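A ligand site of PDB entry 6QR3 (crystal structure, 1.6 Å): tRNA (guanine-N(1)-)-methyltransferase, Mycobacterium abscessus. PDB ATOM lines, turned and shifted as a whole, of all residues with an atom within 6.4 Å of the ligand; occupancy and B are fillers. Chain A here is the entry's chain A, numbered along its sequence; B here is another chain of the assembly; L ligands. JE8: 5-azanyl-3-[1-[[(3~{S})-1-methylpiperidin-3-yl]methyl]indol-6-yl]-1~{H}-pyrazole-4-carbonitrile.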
ATOM      1  N   VAL A  84      20.759   1.888 -27.777  1.00  0.00           N
ATOM      2  CA  VAL A  84      19.836   2.692 -26.978  1.00  0.00           C
ATOM      3  C   VAL A  84      18.549   1.900 -26.724  1.00  0.00           C
ATOM      4  O   VAL A  84      17.696   1.788 -27.610  1.00  0.00           O
ATOM      5  CB  VAL A  84      19.479   4.014 -27.657  1.00  0.00           C
ATOM      6  CG1 VAL A  84      18.649   4.869 -26.727  1.00  0.00           C
ATOM      7  CG2 VAL A  84      20.739   4.753 -28.089  1.00  0.00           C
ATOM      8  N   PRO A  85      18.431   1.287 -25.526  1.00  0.00           N
ATOM      9  CA  PRO A  85      17.160   0.627 -25.245  1.00  0.00           C
ATOM     10  C   PRO A  85      16.007   1.630 -25.257  1.00  0.00           C
ATOM     11  O   PRO A  85      16.158   2.767 -24.785  1.00  0.00           O
ATOM     12  CB  PRO A  85      17.378   0.046 -23.833  1.00  0.00           C
ATOM     13  CG  PRO A  85      18.879  -0.187 -23.772  1.00  0.00           C
ATOM     14  CD  PRO A  85      19.448   1.024 -24.498  1.00  0.00           C
ATOM     15  N   THR A  86      14.871   1.201 -25.813  1.00  0.00           N
ATOM     16  CA  THR A  86      13.676   2.032 -25.833  1.00  0.00           C
ATOM     17  C   THR A  86      12.466   1.164 -26.153  1.00  0.00           C
ATOM     18  O   THR A  86      12.579   0.228 -26.936  1.00  0.00           O
ATOM     19  CB  THR A  86      13.788   3.192 -26.862  1.00  0.00           C
ATOM     20  OG1 THR A  86      12.484   3.728 -27.139  1.00  0.00           O
ATOM     21  CG2 THR A  86      14.460   2.749 -28.159  1.00  0.00           C
ATOM     22  N   PRO A  87      11.318   1.452 -25.544  1.00  0.00           N
ATOM     23  CA  PRO A  87      10.142   0.648 -25.893  1.00  0.00           C
ATOM     24  C   PRO A  87       9.734   0.834 -27.359  1.00  0.00           C
ATOM     25  O   PRO A  87       9.001   0.006 -27.895  1.00  0.00           O
ATOM     26  CB  PRO A  87       9.055   1.147 -24.937  1.00  0.00           C
ATOM     27  CG  PRO A  87       9.545   2.408 -24.383  1.00  0.00           C
ATOM     28  CD  PRO A  87      11.028   2.495 -24.539  1.00  0.00           C
ATOM     29  N   ALA A  88      10.251   1.875 -28.014  1.00  0.00           N
ATOM     30  CA  ALA A  88       9.927   2.114 -29.416  1.00  0.00           C
ATOM     31  C   ALA A  88      11.000   1.558 -30.345  1.00  0.00           C
ATOM     32  O   ALA A  88      11.053   1.908 -31.522  1.00  0.00           O
ATOM     33  CB  ALA A  88       9.737   3.607 -29.675  1.00  0.00           C
ATOM     34  N   CYS A 110      21.462   4.104 -21.230  1.00  0.00           N
ATOM     35  CA  CYS A 110      20.243   3.778 -20.501  1.00  0.00           C
ATOM     36  C   CYS A 110      19.429   5.001 -20.144  1.00  0.00           C
ATOM     37  O   CYS A 110      19.882   5.825 -19.355  1.00  0.00           O
ATOM     38  CB  CYS A 110      20.568   3.027 -19.207  1.00  0.00           C
ATOM     39  SG  CYS A 110      21.412   1.455 -19.493  1.00  0.00           S
ATOM     40  N   GLY A 111      18.229   5.086 -20.705  1.00  0.00           N
ATOM     41  CA  GLY A 111      17.339   6.183 -20.370  1.00  0.00           C
ATOM     42  C   GLY A 111      16.496   5.891 -19.144  1.00  0.00           C
ATOM     43  O   GLY A 111      16.360   4.737 -18.711  1.00  0.00           O
ATOM     44  N   ARG A 112      15.988   6.975 -18.570  1.00  0.00           N
ATOM     45  CA  ARG A 112      14.994   6.941 -17.512  1.00  0.00           C
ATOM     46  C   ARG A 112      13.976   8.029 -17.837  1.00  0.00           C
ATOM     47  O   ARG A 112      14.063   8.648 -18.887  1.00  0.00           O
ATOM     48  CB  ARG A 112      15.630   7.167 -16.135  1.00  0.00           C
ATOM     49  CG  ARG A 112      16.302   5.918 -15.566  1.00  0.00           C
ATOM     50  CD  ARG A 112      15.303   5.107 -14.764  1.00  0.00           C
ATOM     51  NE  ARG A 112      15.740   3.722 -14.665  1.00  0.00           N
ATOM     52  CZ  ARG A 112      15.197   2.818 -13.845  1.00  0.00           C
ATOM     53  NH1 ARG A 112      14.204   3.172 -13.035  1.00  0.00           N
ATOM     54  NH2 ARG A 112      15.660   1.579 -13.839  1.00  0.00           N
ATOM     55  N   TYR A 113      13.028   8.259 -16.918  1.00  0.00           N
ATOM     56  CA  TYR A 113      11.949   9.217 -17.162  1.00  0.00           C
ATOM     57  C   TYR A 113      11.219   8.833 -18.451  1.00  0.00           C
ATOM     58  O   TYR A 113      10.873   7.659 -18.636  1.00  0.00           O
ATOM     59  CB  TYR A 113      12.490  10.654 -17.214  1.00  0.00           C
ATOM     60  CG  TYR A 113      13.340  11.034 -16.012  1.00  0.00           C
ATOM     61  CD1 TYR A 113      12.769  11.602 -14.877  1.00  0.00           C
ATOM     62  CD2 TYR A 113      14.712  10.814 -16.009  1.00  0.00           C
ATOM     63  CE1 TYR A 113      13.536  11.940 -13.775  1.00  0.00           C
ATOM     64  CE2 TYR A 113      15.493  11.153 -14.911  1.00  0.00           C
ATOM     65  CZ  TYR A 113      14.898  11.711 -13.803  1.00  0.00           C
ATOM     66  OH  TYR A 113      15.687  12.047 -12.726  1.00  0.00           O
ATOM     67  N   GLU A 114      10.993   9.791 -19.333  1.00  0.00           N
ATOM     68  CA  GLU A 114      10.286   9.463 -20.583  1.00  0.00           C
ATOM     69  C   GLU A 114      11.224   9.032 -21.680  1.00  0.00           C
ATOM     70  O   GLU A 114      10.798   8.626 -22.760  1.00  0.00           O
ATOM     71  CB  GLU A 114       9.438  10.652 -21.054  1.00  0.00           C
ATOM     72  CG  GLU A 114       8.349  11.041 -20.053  1.00  0.00           C
ATOM     73  CD  GLU A 114       7.338   9.926 -19.834  1.00  0.00           C
ATOM     74  OE1 GLU A 114       7.563   9.057 -18.970  1.00  0.00           O
ATOM     75  OE2 GLU A 114       6.307   9.937 -20.541  1.00  0.00           O
ATOM     76  N   GLY A 115      12.530   9.091 -21.408  1.00  0.00           N
ATOM     77  CA  GLY A 115      13.513   8.716 -22.403  1.00  0.00           C
ATOM     78  C   GLY A 115      14.491   9.831 -22.650  1.00  0.00           C
ATOM     79  O   GLY A 115      14.521  10.802 -21.916  1.00  0.00           O
ATOM     80  N   ILE A 116      15.282   9.691 -23.701  1.00  0.00           N
ATOM     81  CA  ILE A 116      16.346  10.647 -24.017  1.00  0.00           C
ATOM     82  C   ILE A 116      15.924  11.504 -25.185  1.00  0.00           C
ATOM     83  O   ILE A 116      15.355  10.993 -26.151  1.00  0.00           O
ATOM     84  CB  ILE A 116      17.647   9.895 -24.375  1.00  0.00           C
ATOM     85  CG1 ILE A 116      18.008   8.915 -23.247  1.00  0.00           C
ATOM     86  CG2 ILE A 116      18.791  10.880 -24.688  1.00  0.00           C
ATOM     87  CD1 ILE A 116      19.207   8.035 -23.573  1.00  0.00           C
ATOM     88  N   VAL A 133      16.685  -0.249 -29.762  1.00  0.00           N
ATOM     89  CA  VAL A 133      16.119  -1.597 -29.690  1.00  0.00           C
ATOM     90  C   VAL A 133      15.265  -1.779 -28.459  1.00  0.00           C
ATOM     91  O   VAL A 133      15.442  -1.095 -27.453  1.00  0.00           O
ATOM     92  CB  VAL A 133      17.209  -2.715 -29.681  1.00  0.00           C
ATOM     93  CG1 VAL A 133      18.012  -2.704 -30.985  1.00  0.00           C
ATOM     94  CG2 VAL A 133      18.144  -2.549 -28.484  1.00  0.00           C
ATOM     95  N   SER A 134      14.337  -2.731 -28.545  1.00  0.00           N
ATOM     96  CA  SER A 134      13.509  -3.105 -27.413  1.00  0.00           C
ATOM     97  C   SER A 134      13.659  -4.594 -27.116  1.00  0.00           C
ATOM     98  O   SER A 134      13.687  -5.392 -28.049  1.00  0.00           O
ATOM     99  CB  SER A 134      12.045  -2.819 -27.713  1.00  0.00           C
ATOM    100  OG  SER A 134      11.217  -3.376 -26.705  1.00  0.00           O
ATOM    101  N   ILE A 135      13.700  -4.965 -25.831  1.00  0.00           N
ATOM    102  CA  ILE A 135      13.858  -6.383 -25.489  1.00  0.00           C
ATOM    103  C   ILE A 135      12.521  -7.127 -25.382  1.00  0.00           C
ATOM    104  O   ILE A 135      12.509  -8.358 -25.219  1.00  0.00           O
ATOM    105  CB  ILE A 135      14.665  -6.566 -24.177  1.00  0.00           C
ATOM    106  CG1 ILE A 135      13.975  -5.884 -22.998  1.00  0.00           C
ATOM    107  CG2 ILE A 135      16.103  -6.078 -24.363  1.00  0.00           C
ATOM    108  CD1 ILE A 135      14.380  -6.459 -21.653  1.00  0.00           C
ATOM    109  N   GLY A 136      11.397  -6.431 -25.499  1.00  0.00           N
ATOM    110  CA  GLY A 136      10.133  -7.127 -25.467  1.00  0.00           C
ATOM    111  C   GLY A 136       8.941  -6.218 -25.346  1.00  0.00           C
ATOM    112  O   GLY A 136       9.070  -5.012 -25.144  1.00  0.00           O
ATOM    113  N   ASP A 137       7.759  -6.822 -25.455  1.00  0.00           N
ATOM    114  CA  ASP A 137       6.532  -6.035 -25.470  1.00  0.00           C
ATOM    115  C   ASP A 137       5.901  -5.858 -24.105  1.00  0.00           C
ATOM    116  O   ASP A 137       4.788  -6.344 -23.854  1.00  0.00           O
ATOM    117  CB  ASP A 137       5.534  -6.650 -26.445  1.00  0.00           C
ATOM    118  CG  ASP A 137       5.944  -6.470 -27.884  1.00  0.00           C
ATOM    119  OD1 ASP A 137       6.685  -5.503 -28.169  1.00  0.00           O
ATOM    120  OD2 ASP A 137       5.525  -7.286 -28.725  1.00  0.00           O
ATOM    121  N   TYR A 138       6.626  -5.158 -23.255  1.00  0.00           N
ATOM    122  CA  TYR A 138       6.197  -4.798 -21.918  1.00  0.00           C
ATOM    123  C   TYR A 138       6.928  -3.500 -21.628  1.00  0.00           C
ATOM    124  O   TYR A 138       7.878  -3.148 -22.322  1.00  0.00           O
ATOM    125  CB  TYR A 138       6.559  -5.862 -20.880  1.00  0.00           C
ATOM    126  CG  TYR A 138       7.882  -6.513 -21.185  1.00  0.00           C
ATOM    127  CD1 TYR A 138       9.091  -5.866 -20.922  1.00  0.00           C
ATOM    128  CD2 TYR A 138       7.920  -7.754 -21.796  1.00  0.00           C
ATOM    129  CE1 TYR A 138      10.304  -6.460 -21.239  1.00  0.00           C
ATOM    130  CE2 TYR A 138       9.119  -8.368 -22.096  1.00  0.00           C
ATOM    131  CZ  TYR A 138      10.299  -7.718 -21.830  1.00  0.00           C
ATOM    132  OH  TYR A 138      11.493  -8.318 -22.159  1.00  0.00           O
ATOM    133  N   VAL A 139       6.487  -2.818 -20.579  1.00  0.00           N
ATOM    134  CA  VAL A 139       7.032  -1.498 -20.254  1.00  0.00           C
ATOM    135  C   VAL A 139       7.858  -1.566 -18.975  1.00  0.00           C
ATOM    136  O   VAL A 139       7.415  -2.110 -17.963  1.00  0.00           O
ATOM    137  CB  VAL A 139       5.918  -0.470 -20.104  1.00  0.00           C
ATOM    138  CG1 VAL A 139       6.509   0.905 -19.822  1.00  0.00           C
ATOM    139  CG2 VAL A 139       5.064  -0.424 -21.362  1.00  0.00           C
ATOM    140  N   LEU A 140       9.088  -1.082 -19.068  1.00  0.00           N
ATOM    141  CA  LEU A 140       9.988  -0.982 -17.929  1.00  0.00           C
ATOM    142  C   LEU A 140      10.084   0.467 -17.464  1.00  0.00           C
ATOM    143  O   LEU A 140       9.529   1.371 -18.100  1.00  0.00           O
ATOM    144  CB  LEU A 140      11.385  -1.473 -18.309  1.00  0.00           C
ATOM    145  CG  LEU A 140      11.397  -2.908 -18.869  1.00  0.00           C
ATOM    146  CD1 LEU A 140      12.746  -3.195 -19.486  1.00  0.00           C
ATOM    147  CD2 LEU A 140      11.103  -3.904 -17.765  1.00  0.00           C
ATOM    148  N   ASN A 141      10.835   0.700 -16.378  1.00  0.00           N
ATOM    149  CA  ASN A 141      11.043   2.067 -15.882  1.00  0.00           C
ATOM    150  C   ASN A 141      12.181   2.792 -16.597  1.00  0.00           C
ATOM    151  O   ASN A 141      12.318   4.022 -16.493  1.00  0.00           O
ATOM    152  CB  ASN A 141      11.335   2.060 -14.385  1.00  0.00           C
ATOM    153  CG  ASN A 141      10.151   1.609 -13.556  1.00  0.00           C
ATOM    154  OD1 ASN A 141       9.015   1.990 -13.838  1.00  0.00           O
ATOM    155  ND2 ASN A 141      10.414   0.802 -12.540  1.00  0.00           N
ATOM    156  N   GLY A 142      13.017   2.047 -17.303  1.00  0.00           N
ATOM    157  CA  GLY A 142      14.170   2.659 -17.929  1.00  0.00           C
ATOM    158  C   GLY A 142      14.978   1.581 -18.594  1.00  0.00           C
ATOM    159  O   GLY A 142      14.560   0.416 -18.596  1.00  0.00           O
ATOM    160  N   GLY A 143      16.126   1.951 -19.150  1.00  0.00           N
ATOM    161  CA  GLY A 143      16.877   1.025 -19.965  1.00  0.00           C
ATOM    162  C   GLY A 143      17.770   0.033 -19.238  1.00  0.00           C
ATOM    163  O   GLY A 143      18.328  -0.847 -19.879  1.00  0.00           O
ATOM    164  N   GLU A 144      17.916   0.150 -17.918  1.00  0.00           N
ATOM    165  CA  GLU A 144      18.922  -0.659 -17.235  1.00  0.00           C
ATOM    166  C   GLU A 144      18.603  -2.163 -17.304  1.00  0.00           C
ATOM    167  O   GLU A 144      19.492  -2.976 -17.568  1.00  0.00           O
ATOM    168  CB  GLU A 144      19.047  -0.209 -15.775  1.00  0.00           C
ATOM    169  CG  GLU A 144      19.733   1.150 -15.594  1.00  0.00           C
ATOM    170  CD  GLU A 144      18.821   2.346 -15.858  1.00  0.00           C
ATOM    171  OE1 GLU A 144      17.595   2.171 -16.030  1.00  0.00           O
ATOM    172  OE2 GLU A 144      19.355   3.476 -15.885  1.00  0.00           O
ATOM    173  N   ALA A 146      16.937  -3.669 -19.527  1.00  0.00           N
ATOM    174  CA  ALA A 146      17.189  -4.037 -20.917  1.00  0.00           C
ATOM    175  C   ALA A 146      18.692  -4.238 -21.156  1.00  0.00           C
ATOM    176  O   ALA A 146      19.092  -5.184 -21.840  1.00  0.00           O
ATOM    177  CB  ALA A 146      16.634  -2.974 -21.880  1.00  0.00           C
ATOM    178  N   ILE A 150      20.518  -7.496 -22.652  1.00  0.00           N
ATOM    179  CA  ILE A 150      21.336  -7.389 -23.862  1.00  0.00           C
ATOM    180  C   ILE A 150      22.762  -7.843 -23.597  1.00  0.00           C
ATOM    181  O   ILE A 150      23.319  -8.626 -24.378  1.00  0.00           O
ATOM    182  CB  ILE A 150      21.329  -5.942 -24.407  1.00  0.00           C
ATOM    183  CG1 ILE A 150      19.944  -5.633 -24.965  1.00  0.00           C
ATOM    184  CG2 ILE A 150      22.386  -5.765 -25.494  1.00  0.00           C
ATOM    185  CD1 ILE A 150      19.685  -4.139 -25.121  1.00  0.00           C
ATOM    186  N   ARG B 156       5.610  -1.818 -11.372  1.00  0.00           N
ATOM    187  CA  ARG B 156       5.218  -0.464 -11.735  1.00  0.00           C
ATOM    188  C   ARG B 156       3.704  -0.347 -12.022  1.00  0.00           C
ATOM    189  O   ARG B 156       3.176   0.772 -12.149  1.00  0.00           O
ATOM    190  CB  ARG B 156       6.041   0.032 -12.925  1.00  0.00           C
ATOM    191  CG  ARG B 156       5.968  -0.828 -14.166  1.00  0.00           C
ATOM    192  CD  ARG B 156       6.965  -0.316 -15.222  1.00  0.00           C
ATOM    193  NE  ARG B 156       6.726   1.071 -15.612  1.00  0.00           N
ATOM    194  CZ  ARG B 156       5.713   1.480 -16.368  1.00  0.00           C
ATOM    195  NH1 ARG B 156       4.781   0.609 -16.777  1.00  0.00           N
ATOM    196  NH2 ARG B 156       5.582   2.764 -16.701  1.00  0.00           N
ATOM    197  N   GLU B 182       5.952   4.424 -29.058  1.00  0.00           N
ATOM    198  CA  GLU B 182       6.173   5.783 -28.589  1.00  0.00           C
ATOM    199  C   GLU B 182       6.901   6.605 -29.640  1.00  0.00           C
ATOM    200  O   GLU B 182       7.809   6.094 -30.296  1.00  0.00           O
ATOM    201  CB  GLU B 182       7.010   5.816 -27.310  1.00  0.00           C
ATOM    202  CG  GLU B 182       6.518   4.978 -26.156  1.00  0.00           C
ATOM    203  CD  GLU B 182       7.500   5.018 -24.995  1.00  0.00           C
ATOM    204  OE1 GLU B 182       8.619   5.583 -25.163  1.00  0.00           O
ATOM    205  OE2 GLU B 182       7.167   4.492 -23.904  1.00  0.00           O
ATOM    206  N   SER B 185      10.857  12.257 -28.062  1.00  0.00           N
ATOM    207  CA  SER B 185      10.686  13.296 -27.044  1.00  0.00           C
ATOM    208  C   SER B 185      11.822  14.306 -27.161  1.00  0.00           C
ATOM    209  O   SER B 185      12.902  13.966 -27.614  1.00  0.00           O
ATOM    210  CB  SER B 185      10.692  12.688 -25.643  1.00  0.00           C
ATOM    211  OG  SER B 185       9.573  11.840 -25.446  1.00  0.00           O
HETATM  212  C10 JE8 L   1      12.188   3.186 -20.749  1.00  0.00           C
HETATM  213  C13 JE8 L   1      11.789  -0.318 -22.087  1.00  0.00           C
HETATM  214  C15 JE8 L   1      13.523  -1.571 -23.711  1.00  0.00           C
HETATM  215  C17 JE8 L   1      11.183  -2.264 -22.964  1.00  0.00           C
HETATM  216  C21 JE8 L   1      13.692   1.354 -22.305  1.00  0.00           C
HETATM  217  C22 JE8 L   1      14.225   2.617 -22.054  1.00  0.00           C
HETATM  218  C24 JE8 L   1      13.686   4.913 -20.814  1.00  0.00           C
HETATM  219  C01 JE8 L   1       7.826   7.074 -22.150  1.00  0.00           C
HETATM  220  N02 JE8 L   1       7.859   5.940 -21.722  1.00  0.00           N
HETATM  221  C03 JE8 L   1       9.099   5.715 -21.034  1.00  0.00           C
HETATM  222  C04 JE8 L   1       6.665   5.662 -20.989  1.00  0.00           C
HETATM  223  C05 JE8 L   1       6.725   4.449 -20.088  1.00  0.00           C
HETATM  224  C06 JE8 L   1       7.983   4.266 -19.399  1.00  0.00           C
HETATM  225  C07 JE8 L   1       9.127   4.419 -20.250  1.00  0.00           C
HETATM  226  C08 JE8 L   1      10.393   4.276 -19.330  1.00  0.00           C
HETATM  227  N09 JE8 L   1      11.675   4.278 -20.038  1.00  0.00           N
HETATM  228  C11 JE8 L   1      11.638   1.900 -21.013  1.00  0.00           C
HETATM  229  C12 JE8 L   1      12.426   0.986 -21.763  1.00  0.00           C
HETATM  230  C14 JE8 L   1      12.201  -1.331 -22.951  1.00  0.00           C
HETATM  231  N16 JE8 L   1      14.489  -1.805 -24.302  1.00  0.00           N
HETATM  232  N18 JE8 L   1      11.148  -3.494 -23.673  1.00  0.00           N
HETATM  233  N19 JE8 L   1      10.176  -1.813 -22.202  1.00  0.00           N
HETATM  234  N20 JE8 L   1      10.544  -0.598 -21.689  1.00  0.00           N
HETATM  235  C23 JE8 L   1      13.460   3.550 -21.255  1.00  0.00           C
HETATM  236  C25 JE8 L   1      12.553   5.289 -20.047  1.00  0.00           C
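N16 of the ligand lies close to O of Val 133.
O of Pro 85 touches C22 of the ligand (3.3 Å).
Pro 87 touches the ligand.
Gly 111 touches the ligand.
Arg 112 touches the ligand.
Tyr 113 touches the ligand (O to C25, 3.2 Å).
Glu 114 touches the ligand (O to C01, 3.4 Å).
Ile 135 touches the ligand (N to N16, 3.6 Å).
Val 139 touches the ligand.
O of Asn 141 touches C08 of the ligand (3.4 Å).
Gly 142 touches the ligand (CA to C10, 3.5 Å).
Gly 143 touches the ligand.
Ala 146 touches the ligand (CB to N16, 3.4 Å).
Arg 156 of chain B touches the ligand.
Hydrophobic or aromatic side chains that line the ligand: Pro 85, Pro 87, Ile 135, Tyr 138, Val 139, Leu 140 and Ala 146.
Within 4 Å of the ligand: Pro 85, Thr 86, Pro 87, Gly 111, Arg 112, Tyr 113, Glu 114, Val 133, Ser 134, Ile 135, Gly 136, Tyr 138, Val 139, Leu 140, Asn 141, Gly 142, Gly 143, Ala 146, Arg 156 of chain B and Glu 182 of chain B.
O of Tyr 138 sits at hydrogen-bond distance from N19 of the ligand, 2.7 Å away.
A nitrogen (N02) of the ligand is in salt-bridge range of the side-chain carboxylate (OE2) of Glu 182 of chain B (2.7 Å).
The backbone carbonyl oxygen (O) of Gly 136 sits at hydrogen-bond distance from a nitrogen (N18) of the ligand, at 3.0 Å.
The side-chain hydroxyl (OG) of Ser 134 sits at hydrogen-bond distance from a nitrogen (N18) of the ligand, at 3.0 Å.
N20 of the ligand lies within hydrogen-bond range of N of Leu 140.
The backbone NH of Thr 86 is in hydrogen-bond range of a nitrogen (N16) of the ligand (3.4 Å).
The side-chain hydroxyl of Tyr 138 is in hydrogen-bond range of the backbone carbonyl oxygen of Ile 135.
OG of Ser 134 sits at hydrogen-bond distance from O of Gly 136, at 3.1 Å.
O of Val 133 is in hydrogen-bond range of N of Thr 86 (2.9 Å).
The backbone carbonyl oxygen (O) of Val 84 sits at hydrogen-bond distance from the backbone NH (N) of Val 133 (3.1 Å).
OG1 of Thr 86 lies close to N of Ala 88.
The backbone NH (N) of Gly 143 is in hydrogen-bond range of the backbone carbonyl oxygen (O) of Gly 111 (2.8 Å).
OD1 of Asn 141 lies within hydrogen-bond range of NE of Arg 156 of chain B, 3.0 Å away.
The guanidinium group of Arg 112 lies within salt-bridge range of the side-chain carboxylate of Glu 144 (2.8 Å).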
